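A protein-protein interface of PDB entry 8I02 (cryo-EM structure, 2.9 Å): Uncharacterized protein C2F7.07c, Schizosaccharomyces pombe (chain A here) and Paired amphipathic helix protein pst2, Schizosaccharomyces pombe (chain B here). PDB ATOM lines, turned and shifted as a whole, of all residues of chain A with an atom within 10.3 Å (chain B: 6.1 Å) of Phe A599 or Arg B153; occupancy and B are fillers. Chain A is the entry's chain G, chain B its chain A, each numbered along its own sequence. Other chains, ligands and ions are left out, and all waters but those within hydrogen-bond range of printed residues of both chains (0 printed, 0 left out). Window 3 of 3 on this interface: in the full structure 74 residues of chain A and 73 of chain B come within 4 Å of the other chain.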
ATOM      1  N   ILE A 562       9.955 -18.282  -7.368  1.00  0.00           N
ATOM      2  CA  ILE A 562       8.521 -18.050  -7.533  1.00  0.00           C
ATOM      3  C   ILE A 562       8.217 -17.520  -8.928  1.00  0.00           C
ATOM      4  O   ILE A 562       7.300 -17.990  -9.606  1.00  0.00           O
ATOM      5  CB  ILE A 562       8.023 -17.077  -6.460  1.00  0.00           C
ATOM      6  CG1 ILE A 562       7.860 -17.796  -5.137  1.00  0.00           C
ATOM      7  CG2 ILE A 562       6.764 -16.417  -6.909  1.00  0.00           C
ATOM      8  CD1 ILE A 562       7.831 -16.873  -3.988  1.00  0.00           C
ATOM      9  N   LEU A 563       8.981 -16.524  -9.376  1.00  0.00           N
ATOM     10  CA  LEU A 563       8.750 -15.948 -10.694  1.00  0.00           C
ATOM     11  C   LEU A 563       9.026 -16.946 -11.811  1.00  0.00           C
ATOM     12  O   LEU A 563       8.335 -16.940 -12.835  1.00  0.00           O
ATOM     13  CB  LEU A 563       9.607 -14.701 -10.868  1.00  0.00           C
ATOM     14  CG  LEU A 563       9.104 -13.600 -11.794  1.00  0.00           C
ATOM     15  CD1 LEU A 563       9.820 -12.347 -11.467  1.00  0.00           C
ATOM     16  CD2 LEU A 563       9.374 -13.953 -13.234  1.00  0.00           C
ATOM     17  N   CYS A 564      10.034 -17.798 -11.656  1.00  0.00           N
ATOM     18  CA  CYS A 564      10.304 -18.781 -12.696  1.00  0.00           C
ATOM     19  C   CYS A 564       9.219 -19.838 -12.748  1.00  0.00           C
ATOM     20  O   CYS A 564       8.974 -20.430 -13.805  1.00  0.00           O
ATOM     21  CB  CYS A 564      11.661 -19.431 -12.473  1.00  0.00           C
ATOM     22  SG  CYS A 564      11.961 -20.802 -13.589  1.00  0.00           S
ATOM     23  N   ASP A 565       8.571 -20.106 -11.611  1.00  0.00           N
ATOM     24  CA  ASP A 565       7.465 -21.064 -11.608  1.00  0.00           C
ATOM     25  C   ASP A 565       6.209 -20.472 -12.234  1.00  0.00           C
ATOM     26  O   ASP A 565       5.510 -21.147 -12.996  1.00  0.00           O
ATOM     27  CB  ASP A 565       7.174 -21.532 -10.189  1.00  0.00           C
ATOM     28  CG  ASP A 565       5.721 -21.400  -9.835  1.00  0.00           C
ATOM     29  OD1 ASP A 565       5.317 -20.329  -9.367  1.00  0.00           O
ATOM     30  OD2 ASP A 565       4.965 -22.350 -10.054  1.00  0.00           O
ATOM     31  N   VAL A 566       5.906 -19.212 -11.924  1.00  0.00           N
ATOM     32  CA  VAL A 566       4.723 -18.573 -12.489  1.00  0.00           C
ATOM     33  C   VAL A 566       4.881 -18.349 -13.986  1.00  0.00           C
ATOM     34  O   VAL A 566       3.965 -18.612 -14.765  1.00  0.00           O
ATOM     35  CB  VAL A 566       4.440 -17.260 -11.756  1.00  0.00           C
ATOM     36  CG1 VAL A 566       3.503 -16.436 -12.555  1.00  0.00           C
ATOM     37  CG2 VAL A 566       3.852 -17.546 -10.417  1.00  0.00           C
ATOM     38  N   ALA A 567       6.044 -17.864 -14.419  1.00  0.00           N
ATOM     39  CA  ALA A 567       6.236 -17.551 -15.831  1.00  0.00           C
ATOM     40  C   ALA A 567       6.243 -18.796 -16.704  1.00  0.00           C
ATOM     41  O   ALA A 567       5.941 -18.713 -17.897  1.00  0.00           O
ATOM     42  CB  ALA A 567       7.530 -16.770 -16.018  1.00  0.00           C
ATOM     43  N   ASN A 568       6.602 -19.946 -16.150  1.00  0.00           N
ATOM     44  CA  ASN A 568       6.527 -21.204 -16.874  1.00  0.00           C
ATOM     45  C   ASN A 568       5.213 -21.925 -16.642  1.00  0.00           C
ATOM     46  O   ASN A 568       4.979 -22.968 -17.257  1.00  0.00           O
ATOM     47  CB  ASN A 568       7.683 -22.121 -16.478  1.00  0.00           C
ATOM     48  CG  ASN A 568       8.982 -21.734 -17.136  1.00  0.00           C
ATOM     49  OD1 ASN A 568       9.343 -22.269 -18.180  1.00  0.00           O
ATOM     50  ND2 ASN A 568       9.695 -20.798 -16.527  1.00  0.00           N
ATOM     51  N   ASP A 569       4.359 -21.384 -15.772  1.00  0.00           N
ATOM     52  CA  ASP A 569       3.024 -21.917 -15.507  1.00  0.00           C
ATOM     53  C   ASP A 569       3.095 -23.344 -14.971  1.00  0.00           C
ATOM     54  O   ASP A 569       2.634 -24.299 -15.592  1.00  0.00           O
ATOM     55  CB  ASP A 569       2.151 -21.846 -16.754  1.00  0.00           C
ATOM     56  CG  ASP A 569       0.743 -21.483 -16.432  1.00  0.00           C
ATOM     57  OD1 ASP A 569       0.472 -21.162 -15.259  1.00  0.00           O
ATOM     58  OD2 ASP A 569      -0.095 -21.531 -17.350  1.00  0.00           O
ATOM     59  N   ASN A 570       3.697 -23.466 -13.798  1.00  0.00           N
ATOM     60  CA  ASN A 570       3.862 -24.753 -13.134  1.00  0.00           C
ATOM     61  C   ASN A 570       2.624 -24.991 -12.291  1.00  0.00           C
ATOM     62  O   ASN A 570       2.474 -24.421 -11.210  1.00  0.00           O
ATOM     63  CB  ASN A 570       5.125 -24.755 -12.286  1.00  0.00           C
ATOM     64  CG  ASN A 570       5.944 -25.991 -12.476  1.00  0.00           C
ATOM     65  OD1 ASN A 570       5.852 -26.656 -13.504  1.00  0.00           O
ATOM     66  ND2 ASN A 570       6.758 -26.311 -11.486  1.00  0.00           N
ATOM     67  N   LEU A 571       1.721 -25.831 -12.788  1.00  0.00           N
ATOM     68  CA  LEU A 571       0.538 -26.163 -12.010  1.00  0.00           C
ATOM     69  C   LEU A 571       0.850 -27.117 -10.870  1.00  0.00           C
ATOM     70  O   LEU A 571      -0.030 -27.376 -10.045  1.00  0.00           O
ATOM     71  CB  LEU A 571      -0.530 -26.748 -12.928  1.00  0.00           C
ATOM     72  CG  LEU A 571      -1.224 -25.694 -13.781  1.00  0.00           C
ATOM     73  CD1 LEU A 571      -1.936 -26.339 -14.928  1.00  0.00           C
ATOM     74  CD2 LEU A 571      -2.183 -24.906 -12.927  1.00  0.00           C
ATOM     75  N   TYR A 576       0.983 -21.944  -6.216  1.00  0.00           N
ATOM     76  CA  TYR A 576       0.542 -21.164  -7.364  1.00  0.00           C
ATOM     77  C   TYR A 576      -0.964 -21.263  -7.539  1.00  0.00           C
ATOM     78  O   TYR A 576      -1.661 -20.245  -7.633  1.00  0.00           O
ATOM     79  CB  TYR A 576       1.273 -21.675  -8.604  1.00  0.00           C
ATOM     80  CG  TYR A 576       0.977 -21.011  -9.922  1.00  0.00           C
ATOM     81  CD1 TYR A 576       1.161 -21.701 -11.100  1.00  0.00           C
ATOM     82  CD2 TYR A 576       0.551 -19.705 -10.000  1.00  0.00           C
ATOM     83  CE1 TYR A 576       0.915 -21.122 -12.311  1.00  0.00           C
ATOM     84  CE2 TYR A 576       0.298 -19.116 -11.216  1.00  0.00           C
ATOM     85  CZ  TYR A 576       0.485 -19.832 -12.366  1.00  0.00           C
ATOM     86  OH  TYR A 576       0.237 -19.255 -13.582  1.00  0.00           O
ATOM     87  N   LEU A 580      -4.217 -18.716  -7.759  1.00  0.00           N
ATOM     88  CA  LEU A 580      -5.235 -18.790  -8.801  1.00  0.00           C
ATOM     89  C   LEU A 580      -6.639 -18.939  -8.215  1.00  0.00           C
ATOM     90  O   LEU A 580      -7.607 -18.381  -8.742  1.00  0.00           O
ATOM     91  CB  LEU A 580      -4.913 -19.943  -9.740  1.00  0.00           C
ATOM     92  CG  LEU A 580      -3.627 -19.771 -10.531  1.00  0.00           C
ATOM     93  CD1 LEU A 580      -3.467 -20.859 -11.566  1.00  0.00           C
ATOM     94  CD2 LEU A 580      -3.602 -18.428 -11.190  1.00  0.00           C
ATOM     95  N   LEU A 583      -7.861 -15.676  -7.060  1.00  0.00           N
ATOM     96  CA  LEU A 583      -8.382 -14.899  -8.180  1.00  0.00           C
ATOM     97  C   LEU A 583      -9.796 -15.327  -8.557  1.00  0.00           C
ATOM     98  O   LEU A 583     -10.638 -14.482  -8.867  1.00  0.00           O
ATOM     99  CB  LEU A 583      -7.467 -15.023  -9.391  1.00  0.00           C
ATOM    100  CG  LEU A 583      -6.030 -14.577  -9.214  1.00  0.00           C
ATOM    101  CD1 LEU A 583      -5.398 -14.445 -10.569  1.00  0.00           C
ATOM    102  CD2 LEU A 583      -6.016 -13.289  -8.462  1.00  0.00           C
ATOM    103  N   VAL A 595     -13.858 -22.427 -16.055  1.00  0.00           N
ATOM    104  CA  VAL A 595     -12.721 -21.611 -15.632  1.00  0.00           C
ATOM    105  C   VAL A 595     -11.902 -21.288 -16.873  1.00  0.00           C
ATOM    106  O   VAL A 595     -11.993 -22.011 -17.875  1.00  0.00           O
ATOM    107  CB  VAL A 595     -11.857 -22.323 -14.577  1.00  0.00           C
ATOM    108  CG1 VAL A 595     -12.482 -22.228 -13.208  1.00  0.00           C
ATOM    109  CG2 VAL A 595     -11.639 -23.758 -14.971  1.00  0.00           C
ATOM    110  N   PRO A 596     -11.124 -20.214 -16.871  1.00  0.00           N
ATOM    111  CA  PRO A 596     -10.251 -19.931 -18.007  1.00  0.00           C
ATOM    112  C   PRO A 596      -8.855 -20.495 -17.780  1.00  0.00           C
ATOM    113  O   PRO A 596      -8.467 -20.833 -16.662  1.00  0.00           O
ATOM    114  CB  PRO A 596     -10.233 -18.397 -18.051  1.00  0.00           C
ATOM    115  CG  PRO A 596     -10.943 -17.934 -16.777  1.00  0.00           C
ATOM    116  CD  PRO A 596     -11.115 -19.110 -15.905  1.00  0.00           C
ATOM    117  N   ALA A 597      -8.107 -20.603 -18.874  1.00  0.00           N
ATOM    118  CA  ALA A 597      -6.726 -21.061 -18.809  1.00  0.00           C
ATOM    119  C   ALA A 597      -5.978 -20.206 -17.796  1.00  0.00           C
ATOM    120  O   ALA A 597      -6.335 -19.041 -17.600  1.00  0.00           O
ATOM    121  CB  ALA A 597      -6.078 -20.995 -20.190  1.00  0.00           C
ATOM    122  N   PRO A 598      -4.958 -20.736 -17.116  1.00  0.00           N
ATOM    123  CA  PRO A 598      -4.410 -20.009 -15.958  1.00  0.00           C
ATOM    124  C   PRO A 598      -3.810 -18.658 -16.308  1.00  0.00           C
ATOM    125  O   PRO A 598      -3.745 -17.780 -15.440  1.00  0.00           O
ATOM    126  CB  PRO A 598      -3.362 -20.983 -15.404  1.00  0.00           C
ATOM    127  CG  PRO A 598      -3.055 -21.888 -16.513  1.00  0.00           C
ATOM    128  CD  PRO A 598      -4.275 -22.017 -17.332  1.00  0.00           C
ATOM    129  N   PHE A 599      -3.376 -18.465 -17.553  1.00  0.00           N
ATOM    130  CA  PHE A 599      -2.903 -17.164 -18.007  1.00  0.00           C
ATOM    131  C   PHE A 599      -4.049 -16.190 -18.257  1.00  0.00           C
ATOM    132  O   PHE A 599      -3.882 -14.984 -18.046  1.00  0.00           O
ATOM    133  CB  PHE A 599      -2.084 -17.319 -19.288  1.00  0.00           C
ATOM    134  CG  PHE A 599      -0.629 -17.650 -19.061  1.00  0.00           C
ATOM    135  CD1 PHE A 599       0.118 -18.250 -20.060  1.00  0.00           C
ATOM    136  CD2 PHE A 599      -0.005 -17.345 -17.866  1.00  0.00           C
ATOM    137  CE1 PHE A 599       1.442 -18.548 -19.871  1.00  0.00           C
ATOM    138  CE2 PHE A 599       1.324 -17.646 -17.679  1.00  0.00           C
ATOM    139  CZ  PHE A 599       2.043 -18.248 -18.684  1.00  0.00           C
ATOM    140  N   ASP A 600      -5.208 -16.683 -18.708  1.00  0.00           N
ATOM    141  CA  ASP A 600      -6.327 -15.817 -19.072  1.00  0.00           C
ATOM    142  C   ASP A 600      -7.114 -15.349 -17.864  1.00  0.00           C
ATOM    143  O   ASP A 600      -7.782 -14.315 -17.931  1.00  0.00           O
ATOM    144  CB  ASP A 600      -7.255 -16.534 -20.038  1.00  0.00           C
ATOM    145  CG  ASP A 600      -6.562 -16.934 -21.302  1.00  0.00           C
ATOM    146  OD1 ASP A 600      -5.549 -17.653 -21.220  1.00  0.00           O
ATOM    147  OD2 ASP A 600      -7.021 -16.525 -22.383  1.00  0.00           O
ATOM    148  N   LEU A 601      -7.085 -16.101 -16.774  1.00  0.00           N
ATOM    149  CA  LEU A 601      -7.600 -15.587 -15.518  1.00  0.00           C
ATOM    150  C   LEU A 601      -6.732 -14.452 -14.995  1.00  0.00           C
ATOM    151  O   LEU A 601      -7.227 -13.575 -14.279  1.00  0.00           O
ATOM    152  CB  LEU A 601      -7.680 -16.730 -14.513  1.00  0.00           C
ATOM    153  CG  LEU A 601      -8.099 -16.479 -13.076  1.00  0.00           C
ATOM    154  CD1 LEU A 601      -9.548 -16.140 -13.026  1.00  0.00           C
ATOM    155  CD2 LEU A 601      -7.808 -17.715 -12.278  1.00  0.00           C
ATOM    156  N   ALA A 602      -5.455 -14.434 -15.369  1.00  0.00           N
ATOM    157  CA  ALA A 602      -4.522 -13.399 -14.953  1.00  0.00           C
ATOM    158  C   ALA A 602      -4.796 -12.060 -15.614  1.00  0.00           C
ATOM    159  O   ALA A 602      -4.168 -11.066 -15.246  1.00  0.00           O
ATOM    160  CB  ALA A 602      -3.087 -13.838 -15.242  1.00  0.00           C
ATOM    161  N   ASN A 603      -5.701 -12.010 -16.577  1.00  0.00           N
ATOM    162  CA  ASN A 603      -6.225 -10.752 -17.075  1.00  0.00           C
ATOM    163  C   ASN A 603      -7.380 -10.233 -16.228  1.00  0.00           C
ATOM    164  O   ASN A 603      -8.202  -9.448 -16.701  1.00  0.00           O
ATOM    165  CB  ASN A 603      -6.631 -10.913 -18.531  1.00  0.00           C
ATOM    166  CG  ASN A 603      -5.505 -11.455 -19.370  1.00  0.00           C
ATOM    167  OD1 ASN A 603      -4.352 -11.383 -18.971  1.00  0.00           O
ATOM    168  ND2 ASN A 603      -5.827 -12.005 -20.532  1.00  0.00           N
ATOM    169  N   LEU A 604      -7.470 -10.708 -14.988  1.00  0.00           N
ATOM    170  CA  LEU A 604      -8.144  -9.968 -13.933  1.00  0.00           C
ATOM    171  C   LEU A 604      -7.244  -8.871 -13.387  1.00  0.00           C
ATOM    172  O   LEU A 604      -7.734  -7.835 -12.929  1.00  0.00           O
ATOM    173  CB  LEU A 604      -8.536 -10.932 -12.806  1.00  0.00           C
ATOM    174  CG  LEU A 604      -9.318 -10.560 -11.546  1.00  0.00           C
ATOM    175  CD1 LEU A 604      -9.915 -11.817 -11.033  1.00  0.00           C
ATOM    176  CD2 LEU A 604      -8.463  -9.948 -10.478  1.00  0.00           C
ATOM    177  N   LEU A 605      -5.927  -9.086 -13.435  1.00  0.00           N
ATOM    178  CA  LEU A 605      -4.972  -8.190 -12.796  1.00  0.00           C
ATOM    179  C   LEU A 605      -4.714  -6.946 -13.623  1.00  0.00           C
ATOM    180  O   LEU A 605      -4.390  -5.894 -13.063  1.00  0.00           O
ATOM    181  CB  LEU A 605      -3.646  -8.920 -12.534  1.00  0.00           C
ATOM    182  CG  LEU A 605      -3.670 -10.064 -11.513  1.00  0.00           C
ATOM    183  CD1 LEU A 605      -3.772 -11.407 -12.184  1.00  0.00           C
ATOM    184  CD2 LEU A 605      -2.472 -10.024 -10.592  1.00  0.00           C
ATOM    185  N   SER A 606      -4.849  -7.042 -14.936  1.00  0.00           N
ATOM    186  CA  SER A 606      -4.633  -5.898 -15.801  1.00  0.00           C
ATOM    187  C   SER A 606      -5.284  -6.130 -17.157  1.00  0.00           C
ATOM    188  O   SER A 606      -6.441  -5.771 -17.371  1.00  0.00           O
ATOM    189  CB  SER A 606      -3.139  -5.626 -15.959  1.00  0.00           C
ATOM    190  OG  SER A 606      -2.878  -4.250 -16.166  1.00  0.00           O
ATOM    191  N   PHE B 148       3.065  -9.267 -12.655  1.00  0.00           N
ATOM    192  CA  PHE B 148       4.183  -8.882 -13.502  1.00  0.00           C
ATOM    193  C   PHE B 148       4.242  -9.731 -14.766  1.00  0.00           C
ATOM    194  O   PHE B 148       4.471  -9.202 -15.853  1.00  0.00           O
ATOM    195  CB  PHE B 148       5.489  -8.969 -12.712  1.00  0.00           C
ATOM    196  CG  PHE B 148       6.718  -8.682 -13.527  1.00  0.00           C
ATOM    197  CD1 PHE B 148       7.462  -9.707 -14.070  1.00  0.00           C
ATOM    198  CD2 PHE B 148       7.129  -7.391 -13.749  1.00  0.00           C
ATOM    199  CE1 PHE B 148       8.577  -9.452 -14.823  1.00  0.00           C
ATOM    200  CE2 PHE B 148       8.256  -7.136 -14.498  1.00  0.00           C
ATOM    201  CZ  PHE B 148       8.976  -8.170 -15.031  1.00  0.00           C
ATOM    202  N   VAL B 149       4.045 -11.045 -14.657  1.00  0.00           N
ATOM    203  CA  VAL B 149       4.069 -11.834 -15.885  1.00  0.00           C
ATOM    204  C   VAL B 149       2.888 -11.481 -16.773  1.00  0.00           C
ATOM    205  O   VAL B 149       2.999 -11.515 -18.003  1.00  0.00           O
ATOM    206  CB  VAL B 149       4.098 -13.337 -15.577  1.00  0.00           C
ATOM    207  CG1 VAL B 149       4.174 -14.142 -16.868  1.00  0.00           C
ATOM    208  CG2 VAL B 149       5.248 -13.662 -14.668  1.00  0.00           C
ATOM    209  N   SER B 150       1.742 -11.142 -16.178  1.00  0.00           N
ATOM    210  CA  SER B 150       0.600 -10.665 -16.951  1.00  0.00           C
ATOM    211  C   SER B 150       0.991  -9.478 -17.817  1.00  0.00           C
ATOM    212  O   SER B 150       0.868  -9.513 -19.048  1.00  0.00           O
ATOM    213  CB  SER B 150      -0.527 -10.276 -15.996  1.00  0.00           C
ATOM    214  OG  SER B 150      -1.694  -9.919 -16.693  1.00  0.00           O
ATOM    215  N   ARG B 151       1.478  -8.417 -17.175  1.00  0.00           N
ATOM    216  CA  ARG B 151       1.845  -7.203 -17.894  1.00  0.00           C
ATOM    217  C   ARG B 151       2.930  -7.468 -18.925  1.00  0.00           C
ATOM    218  O   ARG B 151       2.888  -6.925 -20.032  1.00  0.00           O
ATOM    219  CB  ARG B 151       2.293  -6.145 -16.901  1.00  0.00           C
ATOM    220  CG  ARG B 151       1.234  -5.838 -15.887  1.00  0.00           C
ATOM    221  CD  ARG B 151       1.519  -4.565 -15.157  1.00  0.00           C
ATOM    222  NE  ARG B 151       2.009  -4.802 -13.810  1.00  0.00           N
ATOM    223  CZ  ARG B 151       1.221  -5.071 -12.775  1.00  0.00           C
ATOM    224  NH1 ARG B 151      -0.089  -5.151 -12.940  1.00  0.00           N
ATOM    225  NH2 ARG B 151       1.743  -5.264 -11.574  1.00  0.00           N
ATOM    226  N   VAL B 152       3.905  -8.314 -18.591  1.00  0.00           N
ATOM    227  CA  VAL B 152       5.014  -8.563 -19.504  1.00  0.00           C
ATOM    228  C   VAL B 152       4.542  -9.315 -20.737  1.00  0.00           C
ATOM    229  O   VAL B 152       4.958  -9.013 -21.858  1.00  0.00           O
ATOM    230  CB  VAL B 152       6.147  -9.315 -18.788  1.00  0.00           C
ATOM    231  CG1 VAL B 152       7.081  -9.933 -19.797  1.00  0.00           C
ATOM    232  CG2 VAL B 152       6.907  -8.381 -17.882  1.00  0.00           C
ATOM    233  N   ARG B 153       3.683 -10.312 -20.563  1.00  0.00           N
ATOM    234  CA  ARG B 153       3.204 -11.024 -21.738  1.00  0.00           C
ATOM    235  C   ARG B 153       2.249 -10.166 -22.542  1.00  0.00           C
ATOM    236  O   ARG B 153       2.100 -10.380 -23.747  1.00  0.00           O
ATOM    237  CB  ARG B 153       2.533 -12.333 -21.334  1.00  0.00           C
ATOM    238  CG  ARG B 153       2.542 -13.391 -22.428  1.00  0.00           C
ATOM    239  CD  ARG B 153       1.918 -14.695 -21.953  1.00  0.00           C
ATOM    240  NE  ARG B 153       0.474 -14.701 -22.130  1.00  0.00           N
ATOM    241  CZ  ARG B 153      -0.389 -14.282 -21.212  1.00  0.00           C
ATOM    242  NH1 ARG B 153       0.046 -13.827 -20.047  1.00  0.00           N
ATOM    243  NH2 ARG B 153      -1.689 -14.320 -21.463  1.00  0.00           N
ATOM    244  N   ARG B 154       1.597  -9.196 -21.894  1.00  0.00           N
ATOM    245  CA  ARG B 154       0.715  -8.271 -22.601  1.00  0.00           C
ATOM    246  C   ARG B 154       1.482  -7.197 -23.359  1.00  0.00           C
ATOM    247  O   ARG B 154       0.963  -6.660 -24.341  1.00  0.00           O
ATOM    248  CB  ARG B 154      -0.251  -7.622 -21.611  1.00  0.00           C
ATOM    249  CG  ARG B 154      -1.170  -6.601 -22.213  1.00  0.00           C
ATOM    250  CD  ARG B 154      -2.015  -5.927 -21.158  1.00  0.00           C
ATOM    251  NE  ARG B 154      -2.826  -6.889 -20.424  1.00  0.00           N
ATOM    252  CZ  ARG B 154      -2.634  -7.200 -19.151  1.00  0.00           C
ATOM    253  NH1 ARG B 154      -1.663  -6.614 -18.479  1.00  0.00           N
ATOM    254  NH2 ARG B 154      -3.413  -8.082 -18.555  1.00  0.00           N
ATOM    255  N   ALA B 155       2.702  -6.876 -22.936  1.00  0.00           N
ATOM    256  CA  ALA B 155       3.498  -5.891 -23.660  1.00  0.00           C
ATOM    257  C   ALA B 155       4.204  -6.482 -24.874  1.00  0.00           C
ATOM    258  O   ALA B 155       4.479  -5.756 -25.833  1.00  0.00           O
ATOM    259  CB  ALA B 155       4.524  -5.257 -22.723  1.00  0.00           C
ATOM    260  N   LEU B 156       4.503  -7.778 -24.865  1.00  0.00           N
ATOM    261  CA  LEU B 156       5.315  -8.401 -25.904  1.00  0.00           C
ATOM    262  C   LEU B 156       4.496  -9.257 -26.864  1.00  0.00           C
ATOM    263  O   LEU B 156       5.051 -10.157 -27.500  1.00  0.00           O
ATOM    264  CB  LEU B 156       6.414  -9.259 -25.274  1.00  0.00           C
ATOM    265  CG  LEU B 156       7.695  -8.634 -24.730  1.00  0.00           C
ATOM    266  CD1 LEU B 156       7.413  -7.777 -23.522  1.00  0.00           C
ATOM    267  CD2 LEU B 156       8.678  -9.725 -24.380  1.00  0.00           C
ATOM    268  N   LEU B 157       3.192  -9.002 -26.982  1.00  0.00           N
ATOM    269  CA  LEU B 157       2.340  -9.891 -27.766  1.00  0.00           C
ATOM    270  C   LEU B 157       2.684  -9.888 -29.247  1.00  0.00           C
ATOM    271  O   LEU B 157       2.273 -10.809 -29.960  1.00  0.00           O
ATOM    272  CB  LEU B 157       0.868  -9.523 -27.590  1.00  0.00           C
ATOM    273  CG  LEU B 157       0.278  -9.597 -26.181  1.00  0.00           C
ATOM    274  CD1 LEU B 157      -0.902  -8.651 -26.053  1.00  0.00           C
ATOM    275  CD2 LEU B 157      -0.142 -11.014 -25.844  1.00  0.00           C
ATOM    276  N   PHE B 163       9.008 -13.393 -25.239  1.00  0.00           N
ATOM    277  CA  PHE B 163       8.546 -13.979 -23.991  1.00  0.00           C
ATOM    278  C   PHE B 163       8.939 -15.436 -23.873  1.00  0.00           C
ATOM    279  O   PHE B 163       8.959 -15.971 -22.763  1.00  0.00           O
ATOM    280  CB  PHE B 163       7.033 -13.862 -23.839  1.00  0.00           C
ATOM    281  CG  PHE B 163       6.531 -14.337 -22.512  1.00  0.00           C
ATOM    282  CD1 PHE B 163       5.771 -15.479 -22.411  1.00  0.00           C
ATOM    283  CD2 PHE B 163       6.840 -13.649 -21.359  1.00  0.00           C
ATOM    284  CE1 PHE B 163       5.317 -15.910 -21.194  1.00  0.00           C
ATOM    285  CE2 PHE B 163       6.388 -14.086 -20.140  1.00  0.00           C
ATOM    286  CZ  PHE B 163       5.626 -15.213 -20.057  1.00  0.00           C
ATOM    287  N   GLN B 167      11.131 -17.059 -20.778  1.00  0.00           N
ATOM    288  CA  GLN B 167      10.684 -18.258 -20.089  1.00  0.00           C
ATOM    289  C   GLN B 167      11.817 -19.262 -19.957  1.00  0.00           C
ATOM    290  O   GLN B 167      12.125 -19.715 -18.852  1.00  0.00           O
ATOM    291  CB  GLN B 167       9.501 -18.880 -20.827  1.00  0.00           C
ATOM    292  CG  GLN B 167       8.162 -18.346 -20.396  1.00  0.00           C
ATOM    293  CD  GLN B 167       7.031 -19.191 -20.906  1.00  0.00           C
ATOM    294  OE1 GLN B 167       7.060 -19.667 -22.036  1.00  0.00           O
ATOM    295  NE2 GLN B 167       6.027 -19.401 -20.067  1.00  0.00           N
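The side-chain hydroxyl (OG) of Ser B150 is in hydrogen-bond range of the backbone carbonyl oxygen (O) of Ala A602 (3.1 Å).
The side-chain amide oxygen of Asn A603 is in hydrogen-bond range of the guanidinium group of Arg B154 (3.5 Å).
The side-chain amide nitrogen (NE2) of Gln B167 sits close to the backbone carbonyl oxygen (O) of Ala A567 (2.3 Å).
NH2 of Arg B154 is in hydrogen-bond range of OG of Ser B150, 3.1 Å away.
O of Cys A564 lies within hydrogen-bond range of ND2 of Asn A568 (2.8 Å).
Val B149 touches Val A566.
Gln B167 touches Asn A568.
Phe A599 touches Arg B153 (CB to NH2, 3.7 Å).
Asn A603 touches Ser B150.
NH2 of Arg B154 touches C of Ser A606, at 3.0 Å.
Printed residues of chain B within 4 Å of Val A566: Val B149.
Printed residues of chain B within 4 Å of Asn A568: Gln B167.
Leu A571 touches none of the printed residues of chain B.
Of the printed residues of chain B, Phe A599 touches Arg B153.
Leu A601 touches none of the printed residues of chain B.
Of the printed residues of chain B, Asn A603 touches Ser B150 (3.8 Å) and Arg B154 (3.5 Å).
Of the printed residues of chain B, Ser A606 touches Arg B154 (3.0 Å).
No residue of chain A comes within 4 Å of Val B152.
No residue of chain A comes within 4 Å of Ala B155.
Of the printed residues of chain A, Gln B167 touches Ala A567 (2.3 Å) and Asn A568 (3.5 Å).
The nearest residue of chain B that does not touch Phe A599 is Gln B167 (4.4 Å).
The nearest residue of chain A that does not touch Arg B153 is Asn A603 (4.7 Å).
Printed residues of chain A that touch a printed residue of chain B: Val A566, Ala A567, Asn A568, Phe A599, Ala A602, Asn A603 and Ser A606.
Hydrophobic or aromatic side chains of chain B that line the printed part of chain A: Val B149.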
